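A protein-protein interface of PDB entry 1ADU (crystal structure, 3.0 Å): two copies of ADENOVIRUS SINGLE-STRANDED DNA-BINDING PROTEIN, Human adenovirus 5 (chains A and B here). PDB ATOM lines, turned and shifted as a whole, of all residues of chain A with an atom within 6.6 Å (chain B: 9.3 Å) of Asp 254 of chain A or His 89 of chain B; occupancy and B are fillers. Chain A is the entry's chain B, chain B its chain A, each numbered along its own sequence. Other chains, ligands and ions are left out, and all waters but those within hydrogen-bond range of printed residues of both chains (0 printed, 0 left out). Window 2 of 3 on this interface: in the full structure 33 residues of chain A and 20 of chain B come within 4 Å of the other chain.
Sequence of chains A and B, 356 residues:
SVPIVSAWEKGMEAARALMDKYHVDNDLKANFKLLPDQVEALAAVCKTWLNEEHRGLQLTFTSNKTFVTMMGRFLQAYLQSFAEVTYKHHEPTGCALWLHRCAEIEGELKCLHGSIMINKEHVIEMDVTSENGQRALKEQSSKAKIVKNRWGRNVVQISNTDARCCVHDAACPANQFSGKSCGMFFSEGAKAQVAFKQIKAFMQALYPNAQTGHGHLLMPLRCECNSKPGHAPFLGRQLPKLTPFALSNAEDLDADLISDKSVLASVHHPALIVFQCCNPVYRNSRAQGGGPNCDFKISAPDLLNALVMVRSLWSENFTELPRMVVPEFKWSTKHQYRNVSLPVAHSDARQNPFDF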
ATOM      1  N   ALA A 250     -20.955 -21.047 -24.413  1.00  0.00           N
ATOM      2  CA  ALA A 250     -22.128 -21.248 -23.568  1.00  0.00           C
ATOM      3  C   ALA A 250     -21.828 -22.179 -22.397  1.00  0.00           C
ATOM      4  O   ALA A 250     -22.436 -22.069 -21.330  1.00  0.00           O
ATOM      5  CB  ALA A 250     -23.289 -21.799 -24.391  1.00  0.00           C
ATOM      6  N   ASP A 252     -19.425 -22.197 -20.392  1.00  0.00           N
ATOM      7  CA  ASP A 252     -18.842 -21.543 -19.222  1.00  0.00           C
ATOM      8  C   ASP A 252     -19.586 -20.287 -18.749  1.00  0.00           C
ATOM      9  O   ASP A 252     -18.974 -19.248 -18.484  1.00  0.00           O
ATOM     10  CB  ASP A 252     -17.351 -21.247 -19.453  1.00  0.00           C
ATOM     11  CG  ASP A 252     -17.085 -20.556 -20.784  1.00  0.00           C
ATOM     12  OD1 ASP A 252     -17.041 -21.258 -21.821  1.00  0.00           O
ATOM     13  OD2 ASP A 252     -16.917 -19.316 -20.793  1.00  0.00           O
ATOM     14  N   LEU A 253     -20.908 -20.392 -18.639  1.00  0.00           N
ATOM     15  CA  LEU A 253     -21.738 -19.277 -18.182  1.00  0.00           C
ATOM     16  C   LEU A 253     -22.556 -19.784 -16.994  1.00  0.00           C
ATOM     17  O   LEU A 253     -23.039 -20.918 -17.016  1.00  0.00           O
ATOM     18  CB  LEU A 253     -22.673 -18.792 -19.301  1.00  0.00           C
ATOM     19  CG  LEU A 253     -22.059 -18.287 -20.613  1.00  0.00           C
ATOM     20  CD1 LEU A 253     -23.149 -17.874 -21.583  1.00  0.00           C
ATOM     21  CD2 LEU A 253     -21.138 -17.123 -20.351  1.00  0.00           C
ATOM     22  N   ASP A 254     -22.692 -18.965 -15.954  1.00  0.00           N
ATOM     23  CA  ASP A 254     -23.444 -19.371 -14.768  1.00  0.00           C
ATOM     24  C   ASP A 254     -24.939 -19.445 -15.063  1.00  0.00           C
ATOM     25  O   ASP A 254     -25.599 -18.430 -15.279  1.00  0.00           O
ATOM     26  CB  ASP A 254     -23.174 -18.417 -13.600  1.00  0.00           C
ATOM     27  CG  ASP A 254     -23.384 -19.075 -12.238  1.00  0.00           C
ATOM     28  OD1 ASP A 254     -24.426 -19.741 -12.037  1.00  0.00           O
ATOM     29  OD2 ASP A 254     -22.501 -18.919 -11.365  1.00  0.00           O
ATOM     30  N   ALA A 255     -25.466 -20.662 -15.000  1.00  0.00           N
ATOM     31  CA  ALA A 255     -26.870 -20.954 -15.274  1.00  0.00           C
ATOM     32  C   ALA A 255     -27.898 -20.129 -14.511  1.00  0.00           C
ATOM     33  O   ALA A 255     -29.074 -20.128 -14.865  1.00  0.00           O
ATOM     34  CB  ALA A 255     -27.137 -22.441 -15.066  1.00  0.00           C
ATOM     35  N   ASP A 256     -27.476 -19.467 -13.442  1.00  0.00           N
ATOM     36  CA  ASP A 256     -28.393 -18.643 -12.660  1.00  0.00           C
ATOM     37  C   ASP A 256     -28.330 -17.207 -13.182  1.00  0.00           C
ATOM     38  O   ASP A 256     -28.388 -16.246 -12.408  1.00  0.00           O
ATOM     39  CB  ASP A 256     -28.018 -18.695 -11.175  1.00  0.00           C
ATOM     40  CG  ASP A 256     -28.037 -20.108 -10.616  1.00  0.00           C
ATOM     41  OD1 ASP A 256     -29.108 -20.547 -10.146  1.00  0.00           O
ATOM     42  OD2 ASP A 256     -26.983 -20.780 -10.650  1.00  0.00           O
ATOM     43  N   LEU A 257     -28.209 -17.076 -14.501  1.00  0.00           N
ATOM     44  CA  LEU A 257     -28.113 -15.773 -15.150  1.00  0.00           C
ATOM     45  C   LEU A 257     -29.453 -15.109 -15.450  1.00  0.00           C
ATOM     46  O   LEU A 257     -30.516 -15.593 -15.047  1.00  0.00           O
ATOM     47  CB  LEU A 257     -27.269 -15.871 -16.432  1.00  0.00           C
ATOM     48  CG  LEU A 257     -27.719 -16.707 -17.635  1.00  0.00           C
ATOM     49  CD1 LEU A 257     -28.642 -15.907 -18.543  1.00  0.00           C
ATOM     50  CD2 LEU A 257     -26.487 -17.122 -18.413  1.00  0.00           C
ATOM     51  N   ILE A 258     -29.367 -13.991 -16.173  1.00  0.00           N
ATOM     52  CA  ILE A 258     -30.517 -13.179 -16.574  1.00  0.00           C
ATOM     53  C   ILE A 258     -31.771 -14.002 -16.871  1.00  0.00           C
ATOM     54  O   ILE A 258     -31.700 -15.086 -17.438  1.00  0.00           O
ATOM     55  CB  ILE A 258     -30.150 -12.255 -17.772  1.00  0.00           C
ATOM     56  CG1 ILE A 258     -29.016 -11.305 -17.354  1.00  0.00           C
ATOM     57  CG2 ILE A 258     -31.370 -11.460 -18.241  1.00  0.00           C
ATOM     58  CD1 ILE A 258     -28.391 -10.517 -18.486  1.00  0.00           C
ATOM     59  N   LEU A 264     -31.240 -19.465 -21.547  1.00  0.00           N
ATOM     60  CA  LEU A 264     -30.993 -20.445 -20.510  1.00  0.00           C
ATOM     61  C   LEU A 264     -31.013 -21.855 -21.084  1.00  0.00           C
ATOM     62  O   LEU A 264     -30.399 -22.766 -20.522  1.00  0.00           O
ATOM     63  CB  LEU A 264     -32.038 -20.299 -19.407  1.00  0.00           C
ATOM     64  CG  LEU A 264     -31.532 -20.534 -17.985  1.00  0.00           C
ATOM     65  CD1 LEU A 264     -30.239 -19.755 -17.764  1.00  0.00           C
ATOM     66  CD2 LEU A 264     -32.604 -20.113 -16.989  1.00  0.00           C
ATOM     67  N   VAL A 267     -27.551 -22.535 -22.515  1.00  0.00           N
ATOM     68  CA  VAL A 267     -26.638 -22.705 -21.387  1.00  0.00           C
ATOM     69  C   VAL A 267     -26.809 -24.087 -20.748  1.00  0.00           C
ATOM     70  O   VAL A 267     -25.828 -24.726 -20.371  1.00  0.00           O
ATOM     71  CB  VAL A 267     -26.847 -21.592 -20.325  1.00  0.00           C
ATOM     72  CG1 VAL A 267     -25.833 -21.729 -19.199  1.00  0.00           C
ATOM     73  CG2 VAL A 267     -26.713 -20.226 -20.970  1.00  0.00           C
ATOM     74  N   PRO B  36     -27.728  -4.914  -4.270  1.00  0.00           N
ATOM     75  CA  PRO B  36     -26.598  -4.704  -5.179  1.00  0.00           C
ATOM     76  C   PRO B  36     -26.892  -3.910  -6.447  1.00  0.00           C
ATOM     77  O   PRO B  36     -26.002  -3.256  -6.990  1.00  0.00           O
ATOM     78  CB  PRO B  36     -26.157  -6.129  -5.500  1.00  0.00           C
ATOM     79  CG  PRO B  36     -27.427  -6.885  -5.418  1.00  0.00           C
ATOM     80  CD  PRO B  36     -28.020  -6.354  -4.152  1.00  0.00           C
ATOM     81  N   ASP B  37     -28.123  -3.983  -6.930  1.00  0.00           N
ATOM     82  CA  ASP B  37     -28.503  -3.275  -8.151  1.00  0.00           C
ATOM     83  C   ASP B  37     -29.030  -1.863  -7.895  1.00  0.00           C
ATOM     84  O   ASP B  37     -29.182  -1.068  -8.828  1.00  0.00           O
ATOM     85  CB  ASP B  37     -29.536  -4.093  -8.931  1.00  0.00           C
ATOM     86  CG  ASP B  37     -30.759  -4.439  -8.100  1.00  0.00           C
ATOM     87  OD1 ASP B  37     -30.615  -5.184  -7.099  1.00  0.00           O
ATOM     88  OD2 ASP B  37     -31.862  -3.961  -8.449  1.00  0.00           O
ATOM     89  N   GLN B  76     -21.400   2.999  -2.983  1.00  0.00           N
ATOM     90  CA  GLN B  76     -22.025   1.727  -2.613  1.00  0.00           C
ATOM     91  C   GLN B  76     -20.978   0.846  -1.953  1.00  0.00           C
ATOM     92  O   GLN B  76     -21.202   0.278  -0.878  1.00  0.00           O
ATOM     93  CB  GLN B  76     -22.575   1.008  -3.844  1.00  0.00           C
ATOM     94  CG  GLN B  76     -23.242  -0.320  -3.513  1.00  0.00           C
ATOM     95  CD  GLN B  76     -23.706  -1.078  -4.740  1.00  0.00           C
ATOM     96  OE1 GLN B  76     -22.978  -1.918  -5.279  1.00  0.00           O
ATOM     97  NE2 GLN B  76     -24.924  -0.795  -5.186  1.00  0.00           N
ATOM     98  N   GLN B  80     -21.170  -0.583   1.843  1.00  0.00           N
ATOM     99  CA  GLN B  80     -21.115  -2.021   2.088  1.00  0.00           C
ATOM    100  C   GLN B  80     -19.928  -2.389   2.984  1.00  0.00           C
ATOM    101  O   GLN B  80     -20.055  -3.243   3.862  1.00  0.00           O
ATOM    102  CB  GLN B  80     -21.026  -2.790   0.768  1.00  0.00           C
ATOM    103  CG  GLN B  80     -22.323  -2.841  -0.030  1.00  0.00           C
ATOM    104  CD  GLN B  80     -22.202  -3.686  -1.294  1.00  0.00           C
ATOM    105  OE1 GLN B  80     -22.711  -3.318  -2.359  1.00  0.00           O
ATOM    106  NE2 GLN B  80     -21.533  -4.826  -1.180  1.00  0.00           N
ATOM    107  N   THR B  86     -21.480  -8.275   2.132  1.00  0.00           N
ATOM    108  CA  THR B  86     -20.985  -8.713   0.836  1.00  0.00           C
ATOM    109  C   THR B  86     -22.048  -9.586   0.195  1.00  0.00           C
ATOM    110  O   THR B  86     -22.777 -10.300   0.888  1.00  0.00           O
ATOM    111  CB  THR B  86     -19.679  -9.504   0.977  1.00  0.00           C
ATOM    112  OG1 THR B  86     -19.691 -10.224   2.216  1.00  0.00           O
ATOM    113  CG2 THR B  86     -18.486  -8.563   0.949  1.00  0.00           C
ATOM    114  N   TYR B  87     -22.176  -9.486  -1.120  1.00  0.00           N
ATOM    115  CA  TYR B  87     -23.165 -10.272  -1.838  1.00  0.00           C
ATOM    116  C   TYR B  87     -22.472 -11.184  -2.834  1.00  0.00           C
ATOM    117  O   TYR B  87     -21.550 -10.761  -3.533  1.00  0.00           O
ATOM    118  CB  TYR B  87     -24.148  -9.362  -2.583  1.00  0.00           C
ATOM    119  CG  TYR B  87     -25.035  -8.520  -1.691  1.00  0.00           C
ATOM    120  CD1 TYR B  87     -25.584  -9.045  -0.522  1.00  0.00           C
ATOM    121  CD2 TYR B  87     -25.331  -7.197  -2.024  1.00  0.00           C
ATOM    122  CE1 TYR B  87     -26.405  -8.275   0.296  1.00  0.00           C
ATOM    123  CE2 TYR B  87     -26.149  -6.420  -1.213  1.00  0.00           C
ATOM    124  CZ  TYR B  87     -26.685  -6.965  -0.055  1.00  0.00           C
ATOM    125  OH  TYR B  87     -27.513  -6.209   0.742  1.00  0.00           O
ATOM    126  N   LYS B  88     -22.893 -12.443  -2.873  1.00  0.00           N
ATOM    127  CA  LYS B  88     -22.315 -13.390  -3.805  1.00  0.00           C
ATOM    128  C   LYS B  88     -22.751 -12.953  -5.193  1.00  0.00           C
ATOM    129  O   LYS B  88     -23.898 -12.553  -5.391  1.00  0.00           O
ATOM    130  CB  LYS B  88     -22.799 -14.808  -3.505  1.00  0.00           C
ATOM    131  CG  LYS B  88     -22.367 -15.320  -2.134  1.00  0.00           C
ATOM    132  CD  LYS B  88     -22.417 -16.842  -2.057  1.00  0.00           C
ATOM    133  CE  LYS B  88     -21.781 -17.357  -0.768  1.00  0.00           C
ATOM    134  NZ  LYS B  88     -21.647 -18.843  -0.777  1.00  0.00           N
ATOM    135  N   HIS B  89     -21.820 -13.001  -6.139  1.00  0.00           N
ATOM    136  CA  HIS B  89     -22.091 -12.600  -7.517  1.00  0.00           C
ATOM    137  C   HIS B  89     -22.304 -11.085  -7.607  1.00  0.00           C
ATOM    138  O   HIS B  89     -23.234 -10.618  -8.274  1.00  0.00           O
ATOM    139  CB  HIS B  89     -23.327 -13.329  -8.084  1.00  0.00           C
ATOM    140  CG  HIS B  89     -23.150 -14.807  -8.256  1.00  0.00           C
ATOM    141  ND1 HIS B  89     -24.218 -15.676  -8.311  1.00  0.00           N
ATOM    142  CD2 HIS B  89     -22.039 -15.567  -8.404  1.00  0.00           C
ATOM    143  CE1 HIS B  89     -23.776 -16.907  -8.487  1.00  0.00           C
ATOM    144  NE2 HIS B  89     -22.457 -16.869  -8.546  1.00  0.00           N
ATOM    145  N   HIS B  90     -21.452 -10.323  -6.924  1.00  0.00           N
ATOM    146  CA  HIS B  90     -21.549  -8.863  -6.946  1.00  0.00           C
ATOM    147  C   HIS B  90     -20.315  -8.168  -6.396  1.00  0.00           C
ATOM    148  O   HIS B  90     -19.856  -8.467  -5.295  1.00  0.00           O
ATOM    149  CB  HIS B  90     -22.780  -8.373  -6.174  1.00  0.00           C
ATOM    150  CG  HIS B  90     -22.867  -6.880  -6.059  1.00  0.00           C
ATOM    151  ND1 HIS B  90     -23.027  -6.054  -7.152  1.00  0.00           N
ATOM    152  CD2 HIS B  90     -22.816  -6.066  -4.978  1.00  0.00           C
ATOM    153  CE1 HIS B  90     -23.073  -4.796  -6.750  1.00  0.00           C
ATOM    154  NE2 HIS B  90     -22.942  -4.777  -5.435  1.00  0.00           N
ATOM    155  N   GLU B  91     -19.797  -7.223  -7.170  1.00  0.00           N
ATOM    156  CA  GLU B  91     -18.640  -6.445  -6.771  1.00  0.00           C
ATOM    157  C   GLU B  91     -19.101  -5.019  -7.043  1.00  0.00           C
ATOM    158  O   GLU B  91     -19.245  -4.610  -8.195  1.00  0.00           O
ATOM    159  CB  GLU B  91     -17.429  -6.816  -7.626  1.00  0.00           C
ATOM    160  CG  GLU B  91     -16.091  -6.522  -6.968  1.00  0.00           C
ATOM    161  CD  GLU B  91     -15.787  -5.047  -6.906  1.00  0.00           C
ATOM    162  OE1 GLU B  91     -15.584  -4.450  -7.984  1.00  0.00           O
ATOM    163  OE2 GLU B  91     -15.749  -4.489  -5.787  1.00  0.00           O
ATOM    164  N   PRO B  92     -19.376  -4.255  -5.976  1.00  0.00           N
ATOM    165  CA  PRO B  92     -19.846  -2.869  -6.028  1.00  0.00           C
ATOM    166  C   PRO B  92     -19.130  -1.881  -6.933  1.00  0.00           C
ATOM    167  O   PRO B  92     -19.784  -1.160  -7.678  1.00  0.00           O
ATOM    168  CB  PRO B  92     -19.798  -2.433  -4.565  1.00  0.00           C
ATOM    169  CG  PRO B  92     -18.735  -3.296  -3.976  1.00  0.00           C
ATOM    170  CD  PRO B  92     -19.047  -4.630  -4.591  1.00  0.00           C
ATOM    171  N   ARG B 222     -16.992  -3.203 -16.099  1.00  0.00           N
ATOM    172  CA  ARG B 222     -18.315  -3.226 -16.715  1.00  0.00           C
ATOM    173  C   ARG B 222     -18.886  -1.860 -17.062  1.00  0.00           C
ATOM    174  O   ARG B 222     -18.819  -0.927 -16.262  1.00  0.00           O
ATOM    175  CB  ARG B 222     -19.298  -3.979 -15.823  1.00  0.00           C
ATOM    176  CG  ARG B 222     -19.584  -3.312 -14.515  1.00  0.00           C
ATOM    177  CD  ARG B 222     -20.626  -4.082 -13.730  1.00  0.00           C
ATOM    178  NE  ARG B 222     -20.027  -5.070 -12.845  1.00  0.00           N
ATOM    179  CZ  ARG B 222     -20.062  -4.991 -11.518  1.00  0.00           C
ATOM    180  NH1 ARG B 222     -20.672  -3.968 -10.927  1.00  0.00           N
ATOM    181  NH2 ARG B 222     -19.480  -5.932 -10.781  1.00  0.00           N
ATOM    182  N   PRO B 233     -25.812 -12.828 -22.791  1.00  0.00           N
ATOM    183  CA  PRO B 233     -24.486 -12.233 -23.036  1.00  0.00           C
ATOM    184  C   PRO B 233     -24.547 -11.505 -24.357  1.00  0.00           C
ATOM    185  O   PRO B 233     -25.616 -11.414 -24.956  1.00  0.00           O
ATOM    186  CB  PRO B 233     -23.500 -13.387 -23.100  1.00  0.00           C
ATOM    187  CG  PRO B 233     -24.168 -14.382 -22.162  1.00  0.00           C
ATOM    188  CD  PRO B 233     -25.667 -14.262 -22.489  1.00  0.00           C
ATOM    189  N   LYS B 334     -13.732 -15.739 -18.698  1.00  0.00           N
ATOM    190  CA  LYS B 334     -14.925 -14.912 -18.848  1.00  0.00           C
ATOM    191  C   LYS B 334     -14.727 -13.584 -19.570  1.00  0.00           C
ATOM    192  O   LYS B 334     -15.695 -12.956 -20.000  1.00  0.00           O
ATOM    193  CB  LYS B 334     -15.592 -14.681 -17.487  1.00  0.00           C
ATOM    194  CG  LYS B 334     -14.703 -14.027 -16.437  1.00  0.00           C
ATOM    195  CD  LYS B 334     -15.435 -13.848 -15.105  1.00  0.00           C
ATOM    196  CE  LYS B 334     -16.598 -12.866 -15.217  1.00  0.00           C
ATOM    197  NZ  LYS B 334     -17.414 -12.781 -13.964  1.00  0.00           N
ATOM    198  N   ARG B 338     -16.046 -12.801 -27.412  1.00  0.00           N
ATOM    199  CA  ARG B 338     -17.005 -13.788 -27.892  1.00  0.00           C
ATOM    200  C   ARG B 338     -17.384 -13.529 -29.351  1.00  0.00           C
ATOM    201  O   ARG B 338     -17.922 -12.474 -29.693  1.00  0.00           O
ATOM    202  CB  ARG B 338     -18.263 -13.786 -27.022  1.00  0.00           C
ATOM    203  CG  ARG B 338     -18.055 -14.322 -25.617  1.00  0.00           C
ATOM    204  CD  ARG B 338     -19.343 -14.250 -24.810  1.00  0.00           C
ATOM    205  NE  ARG B 338     -19.846 -15.565 -24.419  1.00  0.00           N
ATOM    206  CZ  ARG B 338     -20.920 -16.148 -24.946  1.00  0.00           C
ATOM    207  NH1 ARG B 338     -21.612 -15.541 -25.906  1.00  0.00           N
ATOM    208  NH2 ARG B 338     -21.327 -17.324 -24.488  1.00  0.00           N
ATOM    209  N   LEU B 342     -25.514 -16.837 -29.069  1.00  0.00           N
ATOM    210  CA  LEU B 342     -26.425 -17.829 -28.519  1.00  0.00           C
ATOM    211  C   LEU B 342     -27.811 -17.430 -29.024  1.00  0.00           C
ATOM    212  O   LEU B 342     -28.142 -16.240 -29.079  1.00  0.00           O
ATOM    213  CB  LEU B 342     -26.382 -17.823 -26.989  1.00  0.00           C
ATOM    214  CG  LEU B 342     -25.040 -18.115 -26.304  1.00  0.00           C
ATOM    215  CD1 LEU B 342     -25.258 -18.246 -24.798  1.00  0.00           C
ATOM    216  CD2 LEU B 342     -24.416 -19.387 -26.866  1.00  0.00           C
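Among the printed residues, merely in contact across the chains: Ala 250 of chain A with Arg 338 of chain B (3.7 Å), Ala 250 of chain A with Leu 342 of chain B (3.6 Å), Leu 253 of chain A with Pro 233 of chain B (3.7 Å), Leu 253 of chain A with Arg 338 of chain B (3.5 Å) and Leu 253 of chain A with Leu 342 of chain B (3.9 Å).
Of chain B, only His 89 comes within 4 Å of Asp 254 of chain A. No residue of chain B comes within 4 Å of Asp 256 of chain A. Of the printed residues of chain A, Pro 233 of chain B touches Leu 253. Printed residues of chain B within 4 Å of Leu 253 of chain A: Pro 233, Arg 338 and Leu 342. Of the printed residues of chain B, Ala 250 of chain A touches Arg 338 and Leu 342. Of the printed residues of chain A, Arg 338 of chain B touches Ala 250 (3.7 Å) and Leu 253 (3.5 Å). Val 267 of chain A touches none of the printed residues of chain B. The nearest residue of chain A that does not touch His 89 of chain B is Asp 256 of chain A (5.3 Å).
The side-chain carboxylate of Asp 254 of chain A sits close to the backbone NH of Asp 256 of chain A (3.4 Å).
No position is printed for both chains. Of the 6 pairs that touch across the chains among the printed residues, none has its exchanged pair printed and touching as well.
Of the 16 printed residues of chain B, 4 touch a printed residue of chain A. Printed residues of chain B that touch a printed residue of chain A: His 89, Pro 233, Arg 338 and Leu 342. Hydrophobic or aromatic side chains of chain B that line the printed part of chain A: His 89, Pro 233 and Leu 342. Along chain B the printed residues that touch a printed residue of chain A span positions 89 to 342. Of the 10 printed residues of chain A, 3 touch a printed residue of chain B. Hydrophobic or aromatic side chains of chain A within 4 Å of the printed part of chain B: Ala 250 and Leu 253.
OD2 of Asp 254 of chain A sits at hydrogen-bond distance from NE2 of His 89 of chain B.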
